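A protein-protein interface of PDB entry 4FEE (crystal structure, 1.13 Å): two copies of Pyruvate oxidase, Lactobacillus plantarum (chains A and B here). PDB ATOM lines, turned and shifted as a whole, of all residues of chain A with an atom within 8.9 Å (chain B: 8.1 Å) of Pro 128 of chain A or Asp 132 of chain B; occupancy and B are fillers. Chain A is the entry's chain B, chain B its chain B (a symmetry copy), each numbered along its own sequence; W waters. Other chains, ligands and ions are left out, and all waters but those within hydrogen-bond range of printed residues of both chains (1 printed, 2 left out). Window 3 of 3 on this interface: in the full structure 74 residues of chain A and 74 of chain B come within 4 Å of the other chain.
The backbone NH (N) of Thr 88 of chain A lies within hydrogen-bond range of the side-chain hydroxyl (OH) of Tyr 130 of chain A.
The side-chain hydroxyl (OH) of Tyr 95 of chain A lies within hydrogen-bond range of the side-chain carboxylate (OD2) of Asp 132 of chain A (2.7 Å).
NE2 of Gln 110 of chain A sits at hydrogen-bond distance from O of Met 124 of chain A, at 2.9 Å.
OH of Tyr 95 of chain B lies within hydrogen-bond range of OD2 of Asp 132 of chain B (2.7 Å).
The guanidinium group (NH1) of Arg 98 of chain B lies within salt-bridge range of the side-chain carboxylate (OD2) of Asp 132 of chain B (3.0 Å).
Thr 88 of chain A touches Phe 419 of chain B (OG1 to CZ, 3.5 Å).
Tyr 95 of chain A touches Ile 129 of chain B.
Phe 419 of chain B touches Met 124 of chain A.
CB of Pro 128 of chain A touches OD1 of Asp 132 of chain B, at 3.4 Å.
Tyr 95 of chain B touches Ile 129 of chain A (OH to CG1, 3.5 Å).
Ile 129 of chain A touches Asp 132 of chain B.
Asp 132 of chain A touches Pro 128 of chain B (OD1 to CB, 3.4 Å).
Ile 129 of chain B touches Asp 132 of chain A.
Pro 128 of chain A touches just one residue of chain B: Asp 132.
Of the printed residues of chain B, Ile 129 of chain A touches Tyr 95 (3.5 Å) and Asp 132 (3.6 Å).
Of the printed residues of chain B, Asp 132 of chain A touches Pro 128 (3.4 Å) and Ile 129 (3.6 Å).
Met 91 of chain B touches none of the printed residues of chain A.
Leu 94 of chain B touches none of the printed residues of chain A.
Of the printed residues of chain A, Tyr 95 of chain B touches Ile 129.
Of the printed residues of chain A, Ile 129 of chain B touches Tyr 95 and Asp 132.
No residue of chain A comes within 4 Å of Ala 131 of chain B.
Asp 132 of chain B touches two residues of chain A.
The nearest printed residue of chain B that does not touch Pro 128 of chain A is Pro 128 of chain B (5.5 Å).
The nearest residue of chain A that does not touch Asp 132 of chain B is Asn 125 of chain A (4.6 Å).
The nearest printed residue of chain B that does not touch Tyr 95 of chain A is Pro 128 of chain B (5.6 Å).
Of the 19 printed residues of chain A, 6 touch a printed residue of chain B.
Printed residues of chain A that touch a printed residue of chain B: Thr 88, Tyr 95, Met 124, Pro 128, Ile 129 and Asp 132.
Hydrophobic or aromatic side chains of chain A within 4 Å of the printed part of chain B: Tyr 95, Met 124, Pro 128 and Ile 129.
Among the printed residues, no Asp or Glu carboxylate lies within 4 Å of a Lys or Arg side-chain nitrogen of the other chain.
Tyr 95 of chain A touches Ile 129 of chain B, and with the chains exchanged Ile 129 of chain A touches Tyr 95 of chain B.
Pro 128 of chain A touches Asp 132 of chain B, and with the chains exchanged Asp 132 of chain A touches Pro 128 of chain B.
Ile 129 of chain A touches Asp 132 of chain B, and with the chains exchanged Asp 132 of chain A touches Ile 129 of chain B.
Positions printed for both chains: 91, 95, 127, 128, 129, 130, 131, 132, 133, 134 and 137.
Water W1 lies within hydrogen-bond range of OD2 of Asp 132 of chain B (2.8 Å), O of Asn 125 of chain A (2.8 Å) and NH2 of Arg 98 of chain B (2.9 Å).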
ATOM      1  N   THR A  88     -19.862  -0.366 -11.460  1.00  0.00           N
ATOM      2  CA  THR A  88     -20.810  -1.221 -12.136  1.00  0.00           C
ATOM      3  C   THR A  88     -20.459  -1.422 -13.617  1.00  0.00           C
ATOM      4  O   THR A  88     -20.787  -2.465 -14.180  1.00  0.00           O
ATOM      5  CB  THR A  88     -22.282  -0.734 -11.972  1.00  0.00           C
ATOM      6  OG1 THR A  88     -22.421   0.600 -12.396  1.00  0.00           O
ATOM      7  CG2 THR A  88     -22.736  -0.805 -10.509  1.00  0.00           C
ATOM      8  N   MET A  91     -18.566  -4.763 -14.663  1.00  0.00           N
ATOM      9  CA  MET A  91     -19.158  -6.085 -14.542  1.00  0.00           C
ATOM     10  C   MET A  91     -18.847  -7.050 -15.662  1.00  0.00           C
ATOM     11  O   MET A  91     -18.507  -8.212 -15.383  1.00  0.00           O
ATOM     12  CB  MET A  91     -20.688  -5.970 -14.398  1.00  0.00           C
ATOM     13  CG  MET A  91     -21.092  -5.591 -13.006  1.00  0.00           C
ATOM     14  SD  MET A  91     -20.517  -6.693 -11.728  1.00  0.00           S
ATOM     15  CE  MET A  91     -21.138  -5.838 -10.285  1.00  0.00           C
ATOM     16  N   TYR A  95     -17.243 -10.644 -14.683  1.00  0.00           N
ATOM     17  CA  TYR A  95     -17.877 -11.920 -14.939  1.00  0.00           C
ATOM     18  C   TYR A  95     -17.059 -12.740 -15.920  1.00  0.00           C
ATOM     19  O   TYR A  95     -16.983 -13.979 -15.801  1.00  0.00           O
ATOM     20  CB  TYR A  95     -19.341 -11.748 -15.454  1.00  0.00           C
ATOM     21  CG  TYR A  95     -20.281 -11.572 -14.310  1.00  0.00           C
ATOM     22  CD1 TYR A  95     -20.846 -12.694 -13.696  1.00  0.00           C
ATOM     23  CD2 TYR A  95     -20.582 -10.334 -13.746  1.00  0.00           C
ATOM     24  CE1 TYR A  95     -21.700 -12.563 -12.616  1.00  0.00           C
ATOM     25  CE2 TYR A  95     -21.385 -10.231 -12.641  1.00  0.00           C
ATOM     26  CZ  TYR A  95     -21.959 -11.343 -12.067  1.00  0.00           C
ATOM     27  OH  TYR A  95     -22.732 -11.192 -10.932  1.00  0.00           O
ATOM     28  N   GLN A 110     -15.488   4.475  -3.008  1.00  0.00           N
ATOM     29  CA  GLN A 110     -16.596   4.660  -2.081  1.00  0.00           C
ATOM     30  C   GLN A 110     -16.422   6.025  -1.422  1.00  0.00           C
ATOM     31  O   GLN A 110     -15.282   6.512  -1.270  1.00  0.00           O
ATOM     32  CB  GLN A 110     -16.662   3.508  -1.088  1.00  0.00           C
ATOM     33  CG  GLN A 110     -17.735   3.577  -0.038  1.00  0.00           C
ATOM     34  CD  GLN A 110     -19.125   3.663  -0.542  1.00  0.00           C
ATOM     35  OE1 GLN A 110     -19.538   4.645  -1.165  1.00  0.00           O
ATOM     36  NE2 GLN A 110     -19.937   2.617  -0.320  1.00  0.00           N
ATOM     37  N   MET A 124     -23.957   4.663  -1.842  1.00  0.00           N
ATOM     38  CA  MET A 124     -24.822   3.512  -1.701  1.00  0.00           C
ATOM     39  C   MET A 124     -24.002   2.442  -0.952  1.00  0.00           C
ATOM     40  O   MET A 124     -22.788   2.510  -0.878  1.00  0.00           O
ATOM     41  CB  MET A 124     -25.358   3.018  -3.042  1.00  0.00           C
ATOM     42  CG  MET A 124     -24.295   2.388  -3.932  1.00  0.00           C
ATOM     43  SD  MET A 124     -24.501   2.757  -5.686  1.00  0.00           S
ATOM     44  CE  MET A 124     -24.248   4.481  -5.744  1.00  0.00           C
ATOM     45  N   ASN A 125     -24.733   1.424  -0.484  1.00  0.00           N
ATOM     46  CA  ASN A 125     -24.034   0.223   0.020  1.00  0.00           C
ATOM     47  C   ASN A 125     -23.580  -0.546  -1.166  1.00  0.00           C
ATOM     48  O   ASN A 125     -24.382  -1.131  -1.912  1.00  0.00           O
ATOM     49  CB  ASN A 125     -25.024  -0.558   0.886  1.00  0.00           C
ATOM     50  CG  ASN A 125     -24.410  -1.877   1.341  1.00  0.00           C
ATOM     51  OD1 ASN A 125     -23.177  -2.092   1.213  1.00  0.00           O
ATOM     52  ND2 ASN A 125     -25.272  -2.749   1.801  1.00  0.00           N
ATOM     53  N   GLU A 126     -22.248  -0.531  -1.450  1.00  0.00           N
ATOM     54  CA  GLU A 126     -21.731  -1.139  -2.650  1.00  0.00           C
ATOM     55  C   GLU A 126     -21.431  -2.592  -2.509  1.00  0.00           C
ATOM     56  O   GLU A 126     -21.280  -3.289  -3.501  1.00  0.00           O
ATOM     57  CB  GLU A 126     -20.480  -0.372  -3.117  1.00  0.00           C
ATOM     58  CG  GLU A 126     -20.799   1.044  -3.638  1.00  0.00           C
ATOM     59  CD  GLU A 126     -19.586   1.702  -4.204  1.00  0.00           C
ATOM     60  OE1 GLU A 126     -18.684   2.005  -3.375  1.00  0.00           O
ATOM     61  OE2 GLU A 126     -19.478   1.864  -5.428  1.00  0.00           O
ATOM     62  N   ASN A 127     -21.348  -3.104  -1.294  1.00  0.00           N
ATOM     63  CA  ASN A 127     -20.945  -4.513  -1.118  1.00  0.00           C
ATOM     64  C   ASN A 127     -21.893  -5.484  -1.831  1.00  0.00           C
ATOM     65  O   ASN A 127     -21.411  -6.439  -2.454  1.00  0.00           O
ATOM     66  CB  ASN A 127     -20.770  -4.790   0.375  1.00  0.00           C
ATOM     67  CG  ASN A 127     -20.120  -6.147   0.608  1.00  0.00           C
ATOM     68  OD1 ASN A 127     -20.814  -7.116   0.953  1.00  0.00           O
ATOM     69  ND2 ASN A 127     -18.824  -6.213   0.406  1.00  0.00           N
ATOM     70  N   PRO A 128     -23.232  -5.320  -1.777  1.00  0.00           N
ATOM     71  CA  PRO A 128     -24.094  -6.291  -2.436  1.00  0.00           C
ATOM     72  C   PRO A 128     -23.950  -6.337  -3.940  1.00  0.00           C
ATOM     73  O   PRO A 128     -24.331  -7.348  -4.552  1.00  0.00           O
ATOM     74  CB  PRO A 128     -25.540  -5.862  -2.053  1.00  0.00           C
ATOM     75  CG  PRO A 128     -25.390  -4.959  -0.888  1.00  0.00           C
ATOM     76  CD  PRO A 128     -24.022  -4.387  -0.932  1.00  0.00           C
ATOM     77  N   ILE A 129     -23.421  -5.282  -4.536  1.00  0.00           N
ATOM     78  CA  ILE A 129     -23.286  -5.241  -5.993  1.00  0.00           C
ATOM     79  C   ILE A 129     -22.389  -6.364  -6.481  1.00  0.00           C
ATOM     80  O   ILE A 129     -22.621  -6.897  -7.564  1.00  0.00           O
ATOM     81  CB  ILE A 129     -22.767  -3.839  -6.411  1.00  0.00           C
ATOM     82  CG1 ILE A 129     -23.685  -2.694  -5.930  1.00  0.00           C
ATOM     83  CG2 ILE A 129     -22.538  -3.763  -7.899  1.00  0.00           C
ATOM     84  CD1 ILE A 129     -23.163  -1.320  -6.275  1.00  0.00           C
ATOM     85  N   TYR A 130     -21.329  -6.633  -5.718  1.00  0.00           N
ATOM     86  CA  TYR A 130     -20.249  -7.521  -6.126  1.00  0.00           C
ATOM     87  C   TYR A 130     -20.303  -8.889  -5.532  1.00  0.00           C
ATOM     88  O   TYR A 130     -19.423  -9.715  -5.789  1.00  0.00           O
ATOM     89  CB  TYR A 130     -18.858  -6.848  -5.868  1.00  0.00           C
ATOM     90  CG  TYR A 130     -18.826  -5.500  -6.567  1.00  0.00           C
ATOM     91  CD1 TYR A 130     -18.508  -5.424  -7.914  1.00  0.00           C
ATOM     92  CD2 TYR A 130     -19.160  -4.334  -5.905  1.00  0.00           C
ATOM     93  CE1 TYR A 130     -18.493  -4.210  -8.585  1.00  0.00           C
ATOM     94  CE2 TYR A 130     -19.210  -3.116  -6.593  1.00  0.00           C
ATOM     95  CZ  TYR A 130     -18.869  -3.061  -7.921  1.00  0.00           C
ATOM     96  OH  TYR A 130     -18.927  -1.902  -8.632  1.00  0.00           O
ATOM     97  N   ALA A 131     -21.338  -9.183  -4.736  1.00  0.00           N
ATOM     98  CA  ALA A 131     -21.365 -10.438  -4.002  1.00  0.00           C
ATOM     99  C   ALA A 131     -21.445 -11.663  -4.889  1.00  0.00           C
ATOM    100  O   ALA A 131     -20.822 -12.678  -4.595  1.00  0.00           O
ATOM    101  CB  ALA A 131     -22.558 -10.423  -3.003  1.00  0.00           C
ATOM    102  N   ASP A 132     -22.156 -11.570  -6.015  1.00  0.00           N
ATOM    103  CA  ASP A 132     -22.265 -12.725  -6.864  1.00  0.00           C
ATOM    104  C   ASP A 132     -21.002 -12.991  -7.682  1.00  0.00           C
ATOM    105  O   ASP A 132     -20.576 -14.140  -7.873  1.00  0.00           O
ATOM    106  CB  ASP A 132     -23.482 -12.582  -7.784  1.00  0.00           C
ATOM    107  CG  ASP A 132     -23.576 -13.790  -8.715  1.00  0.00           C
ATOM    108  OD1 ASP A 132     -23.874 -14.901  -8.220  1.00  0.00           O
ATOM    109  OD2 ASP A 132     -23.382 -13.615  -9.950  1.00  0.00           O
ATOM    110  N   VAL A 133     -20.358 -11.928  -8.195  1.00  0.00           N
ATOM    111  CA  VAL A 133     -19.234 -12.142  -9.105  1.00  0.00           C
ATOM    112  C   VAL A 133     -17.979 -12.551  -8.380  1.00  0.00           C
ATOM    113  O   VAL A 133     -17.110 -13.203  -8.979  1.00  0.00           O
ATOM    114  CB  VAL A 133     -18.976 -10.898  -9.999  1.00  0.00           C
ATOM    115  CG1 VAL A 133     -18.349  -9.739  -9.227  1.00  0.00           C
ATOM    116  CG2 VAL A 133     -18.173 -11.289 -11.230  1.00  0.00           C
ATOM    117  N   ALA A 134     -17.814 -12.134  -7.136  1.00  0.00           N
ATOM    118  CA  ALA A 134     -16.538 -12.127  -6.470  1.00  0.00           C
ATOM    119  C   ALA A 134     -16.302 -13.346  -5.572  1.00  0.00           C
ATOM    120  O   ALA A 134     -17.205 -13.767  -4.844  1.00  0.00           O
ATOM    121  CB  ALA A 134     -16.431 -10.886  -5.605  1.00  0.00           C
ATOM    122  N   ASN A 137     -14.999 -10.238  -1.333  1.00  0.00           N
ATOM    123  CA  ASN A 137     -15.804  -9.031  -1.575  1.00  0.00           C
ATOM    124  C   ASN A 137     -16.012  -8.258  -0.275  1.00  0.00           C
ATOM    125  O   ASN A 137     -16.915  -8.581   0.493  1.00  0.00           O
ATOM    126  CB  ASN A 137     -17.160  -9.420  -2.146  1.00  0.00           C
ATOM    127  CG  ASN A 137     -18.097  -8.238  -2.292  1.00  0.00           C
ATOM    128  OD1 ASN A 137     -17.648  -7.177  -2.718  1.00  0.00           O
ATOM    129  ND2 ASN A 137     -19.374  -8.456  -1.997  1.00  0.00           N
ATOM    130  N   VAL A 138     -15.174  -7.256  -0.043  1.00  0.00           N
ATOM    131  CA  VAL A 138     -15.175  -6.574   1.260  1.00  0.00           C
ATOM    132  C   VAL A 138     -15.108  -5.070   1.073  1.00  0.00           C
ATOM    133  O   VAL A 138     -14.508  -4.551   0.138  1.00  0.00           O
ATOM    134  CB  VAL A 138     -14.042  -7.057   2.165  1.00  0.00           C
ATOM    135  CG1 VAL A 138     -14.142  -8.562   2.442  1.00  0.00           C
ATOM    136  CG2 VAL A 138     -12.686  -6.729   1.585  1.00  0.00           C
ATOM    137  N   THR A 139     -15.738  -4.366   2.026  1.00  0.00           N
ATOM    138  CA  THR A 139     -15.608  -2.937   2.195  1.00  0.00           C
ATOM    139  C   THR A 139     -14.582  -2.682   3.300  1.00  0.00           C
ATOM    140  O   THR A 139     -14.778  -3.081   4.457  1.00  0.00           O
ATOM    141  CB  THR A 139     -16.928  -2.253   2.522  1.00  0.00           C
ATOM    142  OG1 THR A 139     -17.881  -2.395   1.450  1.00  0.00           O
ATOM    143  CG2 THR A 139     -16.733  -0.761   2.716  1.00  0.00           C
ATOM    144  N   GLN A 167     -14.012  -2.572  -1.850  1.00  0.00           N
ATOM    145  CA  GLN A 167     -14.580  -1.237  -1.836  1.00  0.00           C
ATOM    146  C   GLN A 167     -13.796  -0.391  -0.816  1.00  0.00           C
ATOM    147  O   GLN A 167     -13.626  -0.795   0.345  1.00  0.00           O
ATOM    148  CB  GLN A 167     -16.072  -1.220  -1.472  1.00  0.00           C
ATOM    149  CG  GLN A 167     -16.916  -2.082  -2.412  1.00  0.00           C
ATOM    150  CD  GLN A 167     -17.181  -3.484  -1.977  1.00  0.00           C
ATOM    151  OE1 GLN A 167     -17.433  -3.769  -0.801  1.00  0.00           O
ATOM    152  NE2 GLN A 167     -17.165  -4.412  -2.911  1.00  0.00           N
ATOM    153  N   MET B  91     -26.644  -2.862 -16.312  1.00  0.00           N
ATOM    154  CA  MET B  91     -26.555  -2.385 -14.941  1.00  0.00           C
ATOM    155  C   MET B  91     -26.547  -0.884 -14.767  1.00  0.00           C
ATOM    156  O   MET B  91     -27.273  -0.372 -13.898  1.00  0.00           O
ATOM    157  CB  MET B  91     -25.305  -2.970 -14.256  1.00  0.00           C
ATOM    158  CG  MET B  91     -25.518  -4.387 -13.817  1.00  0.00           C
ATOM    159  SD  MET B  91     -26.897  -4.634 -12.714  1.00  0.00           S
ATOM    160  CE  MET B  91     -26.825  -6.412 -12.529  1.00  0.00           C
ATOM    161  N   LEU B  94     -30.015   0.306 -15.011  1.00  0.00           N
ATOM    162  CA  LEU B  94     -30.877  -0.178 -13.950  1.00  0.00           C
ATOM    163  C   LEU B  94     -30.593   0.532 -12.631  1.00  0.00           C
ATOM    164  O   LEU B  94     -31.516   0.888 -11.909  1.00  0.00           O
ATOM    165  CB  LEU B  94     -30.758  -1.696 -13.792  1.00  0.00           C
ATOM    166  CG  LEU B  94     -31.088  -2.506 -15.061  1.00  0.00           C
ATOM    167  CD1 LEU B  94     -31.009  -3.981 -14.744  1.00  0.00           C
ATOM    168  CD2 LEU B  94     -32.427  -2.143 -15.664  1.00  0.00           C
ATOM    169  N   TYR B  95     -29.314   0.754 -12.297  1.00  0.00           N
ATOM    170  CA  TYR B  95     -29.001   1.493 -11.091  1.00  0.00           C
ATOM    171  C   TYR B  95     -29.446   2.939 -11.215  1.00  0.00           C
ATOM    172  O   TYR B  95     -29.896   3.550 -10.225  1.00  0.00           O
ATOM    173  CB  TYR B  95     -27.481   1.414 -10.741  1.00  0.00           C
ATOM    174  CG  TYR B  95     -27.181   0.163  -9.988  1.00  0.00           C
ATOM    175  CD1 TYR B  95     -27.294   0.147  -8.594  1.00  0.00           C
ATOM    176  CD2 TYR B  95     -26.863  -1.047 -10.602  1.00  0.00           C
ATOM    177  CE1 TYR B  95     -27.049  -1.006  -7.871  1.00  0.00           C
ATOM    178  CE2 TYR B  95     -26.680  -2.190  -9.871  1.00  0.00           C
ATOM    179  CZ  TYR B  95     -26.764  -2.182  -8.497  1.00  0.00           C
ATOM    180  OH  TYR B  95     -26.607  -3.368  -7.805  1.00  0.00           O
ATOM    181  N   ARG B  98     -33.077   2.814 -10.334  1.00  0.00           N
ATOM    182  CA  ARG B  98     -33.291   2.614  -8.900  1.00  0.00           C
ATOM    183  C   ARG B  98     -33.067   3.930  -8.166  1.00  0.00           C
ATOM    184  O   ARG B  98     -33.899   4.365  -7.352  1.00  0.00           O
ATOM    185  CB  ARG B  98     -32.356   1.558  -8.348  1.00  0.00           C
ATOM    186  CG  ARG B  98     -32.579   1.303  -6.860  1.00  0.00           C
ATOM    187  CD  ARG B  98     -31.658   0.325  -6.191  1.00  0.00           C
ATOM    188  NE  ARG B  98     -30.372   0.940  -5.931  1.00  0.00           N
ATOM    189  CZ  ARG B  98     -29.345   0.333  -5.344  1.00  0.00           C
ATOM    190  NH1 ARG B  98     -29.437  -0.964  -5.087  1.00  0.00           N
ATOM    191  NH2 ARG B  98     -28.256   0.993  -5.084  1.00  0.00           N
ATOM    192  N   GLU B  99     -31.949   4.590  -8.435  1.00  0.00           N
ATOM    193  CA  GLU B  99     -31.576   5.769  -7.681  1.00  0.00           C
ATOM    194  C   GLU B  99     -32.434   6.972  -8.010  1.00  0.00           C
ATOM    195  O   GLU B  99     -32.675   7.789  -7.121  1.00  0.00           O
ATOM    196  CB  GLU B  99     -30.095   6.056  -7.843  1.00  0.00           C
ATOM    197  CG  GLU B  99     -29.153   4.975  -7.291  1.00  0.00           C
ATOM    198  CD  GLU B  99     -29.350   4.772  -5.825  1.00  0.00           C
ATOM    199  OE1 GLU B  99     -29.317   5.741  -5.050  1.00  0.00           O
ATOM    200  OE2 GLU B  99     -29.541   3.631  -5.397  1.00  0.00           O
ATOM    201  N   ASN B 127     -30.148 -15.079 -11.050  1.00  0.00           N
ATOM    202  CA  ASN B 127     -30.946 -14.333 -10.058  1.00  0.00           C
ATOM    203  C   ASN B 127     -30.072 -13.486  -9.126  1.00  0.00           C
ATOM    204  O   ASN B 127     -30.439 -12.337  -8.844  1.00  0.00           O
ATOM    205  CB  ASN B 127     -31.869 -15.312  -9.334  1.00  0.00           C
ATOM    206  CG  ASN B 127     -32.887 -14.573  -8.476  1.00  0.00           C
ATOM    207  OD1 ASN B 127     -32.724 -14.495  -7.248  1.00  0.00           O
ATOM    208  ND2 ASN B 127     -33.900 -14.032  -9.113  1.00  0.00           N
ATOM    209  N   PRO B 128     -28.926 -13.976  -8.604  1.00  0.00           N
ATOM    210  CA  PRO B 128     -28.150 -13.149  -7.691  1.00  0.00           C
ATOM    211  C   PRO B 128     -27.577 -11.897  -8.315  1.00  0.00           C
ATOM    212  O   PRO B 128     -27.237 -10.957  -7.578  1.00  0.00           O
ATOM    213  CB  PRO B 128     -27.000 -14.074  -7.199  1.00  0.00           C
ATOM    214  CG  PRO B 128     -27.433 -15.452  -7.525  1.00  0.00           C
ATOM    215  CD  PRO B 128     -28.411 -15.369  -8.636  1.00  0.00           C
ATOM    216  N   ILE B 129     -27.460 -11.868  -9.631  1.00  0.00           N
ATOM    217  CA  ILE B 129     -26.878 -10.704 -10.301  1.00  0.00           C
ATOM    218  C   ILE B 129     -27.702  -9.460 -10.028  1.00  0.00           C
ATOM    219  O   ILE B 129     -27.140  -8.371  -9.924  1.00  0.00           O
ATOM    220  CB  ILE B 129     -26.744 -11.010 -11.817  1.00  0.00           C
ATOM    221  CG1 ILE B 129     -25.893 -12.267 -12.101  1.00  0.00           C
ATOM    222  CG2 ILE B 129     -26.217  -9.816 -12.571  1.00  0.00           C
ATOM    223  CD1 ILE B 129     -25.803 -12.614 -13.567  1.00  0.00           C
ATOM    224  N   TYR B 130     -29.024  -9.630 -10.014  1.00  0.00           N
ATOM    225  CA  TYR B 130     -29.977  -8.530  -9.981  1.00  0.00           C
ATOM    226  C   TYR B 130     -30.576  -8.258  -8.641  1.00  0.00           C
ATOM    227  O   TYR B 130     -31.415  -7.364  -8.504  1.00  0.00           O
ATOM    228  CB  TYR B 130     -31.090  -8.735 -11.065  1.00  0.00           C
ATOM    229  CG  TYR B 130     -30.428  -8.919 -12.420  1.00  0.00           C
ATOM    230  CD1 TYR B 130     -30.042  -7.812 -13.160  1.00  0.00           C
ATOM    231  CD2 TYR B 130     -30.148 -10.175 -12.924  1.00  0.00           C
ATOM    232  CE1 TYR B 130     -29.416  -7.949 -14.390  1.00  0.00           C
ATOM    233  CE2 TYR B 130     -29.458 -10.318 -14.133  1.00  0.00           C
ATOM    234  CZ  TYR B 130     -29.105  -9.208 -14.859  1.00  0.00           C
ATOM    235  OH  TYR B 130     -28.413  -9.302 -16.027  1.00  0.00           O
ATOM    236  N   ALA B 131     -30.158  -9.001  -7.609  1.00  0.00           N
ATOM    237  CA  ALA B 131     -30.815  -8.894  -6.316  1.00  0.00           C
ATOM    238  C   ALA B 131     -30.657  -7.538  -5.660  1.00  0.00           C
ATOM    239  O   ALA B 131     -31.591  -7.043  -5.035  1.00  0.00           O
ATOM    240  CB  ALA B 131     -30.277 -10.009  -5.373  1.00  0.00           C
ATOM    241  N   ASP B 132     -29.505  -6.890  -5.842  1.00  0.00           N
ATOM    242  CA  ASP B 132     -29.322  -5.610  -5.213  1.00  0.00           C
ATOM    243  C   ASP B 132     -30.070  -4.480  -5.919  1.00  0.00           C
ATOM    244  O   ASP B 132     -30.645  -3.581  -5.287  1.00  0.00           O
ATOM    245  CB  ASP B 132     -27.827  -5.286  -5.116  1.00  0.00           C
ATOM    246  CG  ASP B 132     -27.632  -3.909  -4.484  1.00  0.00           C
ATOM    247  OD1 ASP B 132     -27.911  -3.766  -3.271  1.00  0.00           O
ATOM    248  OD2 ASP B 132     -27.167  -2.978  -5.199  1.00  0.00           O
ATOM    249  N   VAL B 133     -30.088  -4.491  -7.263  1.00  0.00           N
ATOM    250  CA  VAL B 133     -30.662  -3.354  -7.981  1.00  0.00           C
ATOM    251  C   VAL B 133     -32.167  -3.366  -7.963  1.00  0.00           C
ATOM    252  O   VAL B 133     -32.791  -2.302  -8.092  1.00  0.00           O
ATOM    253  CB  VAL B 133     -30.127  -3.266  -9.437  1.00  0.00           C
ATOM    254  CG1 VAL B 133     -30.709  -4.350 -10.343  1.00  0.00           C
ATOM    255  CG2 VAL B 133     -30.328  -1.864  -9.991  1.00  0.00           C
ATOM    256  N   ALA B 134     -32.780  -4.536  -7.880  1.00  0.00           N
ATOM    257  CA  ALA B 134     -34.166  -4.725  -8.223  1.00  0.00           C
ATOM    258  C   ALA B 134     -35.111  -4.699  -7.018  1.00  0.00           C
ATOM    259  O   ALA B 134     -34.806  -5.281  -5.974  1.00  0.00           O
ATOM    260  CB  ALA B 134     -34.332  -6.065  -8.913  1.00  0.00           C
ATOM    261  N   ASP B 135     -36.246  -4.075  -7.184  1.00  0.00           N
ATOM    262  CA  ASP B 135     -37.348  -4.193  -6.244  1.00  0.00           C
ATOM    263  C   ASP B 135     -37.998  -5.562  -6.302  1.00  0.00           C
ATOM    264  O   ASP B 135     -38.498  -6.054  -5.279  1.00  0.00           O
ATOM    265  CB  ASP B 135     -38.383  -3.103  -6.550  1.00  0.00           C
ATOM    266  CG  ASP B 135     -39.591  -3.158  -5.659  1.00  0.00           C
ATOM    267  OD1 ASP B 135     -39.455  -2.608  -4.568  1.00  0.00           O
ATOM    268  OD2 ASP B 135     -40.597  -3.755  -6.086  1.00  0.00           O
ATOM    269  N   ASN B 137     -37.372  -9.415  -8.417  1.00  0.00           N
ATOM    270  CA  ASN B 137     -36.260 -10.106  -9.087  1.00  0.00           C
ATOM    271  C   ASN B 137     -36.490 -11.615  -9.088  1.00  0.00           C
ATOM    272  O   ASN B 137     -36.178 -12.284  -8.106  1.00  0.00           O
ATOM    273  CB  ASN B 137     -34.954  -9.801  -8.367  1.00  0.00           C
ATOM    274  CG  ASN B 137     -33.782 -10.588  -8.917  1.00  0.00           C
ATOM    275  OD1 ASN B 137     -33.677 -10.719 -10.134  1.00  0.00           O
ATOM    276  ND2 ASN B 137     -32.905 -11.041  -8.028  1.00  0.00           N
ATOM    277  N   VAL B 163     -37.067  -0.824 -10.137  1.00  0.00           N
ATOM    278  CA  VAL B 163     -36.733  -1.789 -11.159  1.00  0.00           C
ATOM    279  C   VAL B 163     -37.318  -3.162 -10.849  1.00  0.00           C
ATOM    280  O   VAL B 163     -37.121  -3.686  -9.749  1.00  0.00           O
ATOM    281  CB  VAL B 163     -35.206  -1.882 -11.333  1.00  0.00           C
ATOM    282  CG1 VAL B 163     -34.830  -2.926 -12.356  1.00  0.00           C
ATOM    283  CG2 VAL B 163     -34.620  -0.522 -11.724  1.00  0.00           C
ATOM    284  N   PHE B 419     -27.322   8.483  -9.099  1.00  0.00           N
ATOM    285  CA  PHE B 419     -26.298   7.545  -9.485  1.00  0.00           C
ATOM    286  C   PHE B 419     -25.212   8.242 -10.291  1.00  0.00           C
ATOM    287  O   PHE B 419     -24.060   7.859 -10.257  1.00  0.00           O
ATOM    288  CB  PHE B 419     -26.931   6.376 -10.243  1.00  0.00           C
ATOM    289  CG  PHE B 419     -26.057   5.153 -10.438  1.00  0.00           C
ATOM    290  CD1 PHE B 419     -25.538   4.462  -9.324  1.00  0.00           C
ATOM    291  CD2 PHE B 419     -25.770   4.699 -11.698  1.00  0.00           C
ATOM    292  CE1 PHE B 419     -24.753   3.314  -9.536  1.00  0.00           C
ATOM    293  CE2 PHE B 419     -24.989   3.576 -11.873  1.00  0.00           C
ATOM    294  CZ  PHE B 419     -24.461   2.891 -10.799  1.00  0.00           C
HETATM  295  O   HOH W   1     -26.210  -0.693  -3.995  1.00  0.00           O
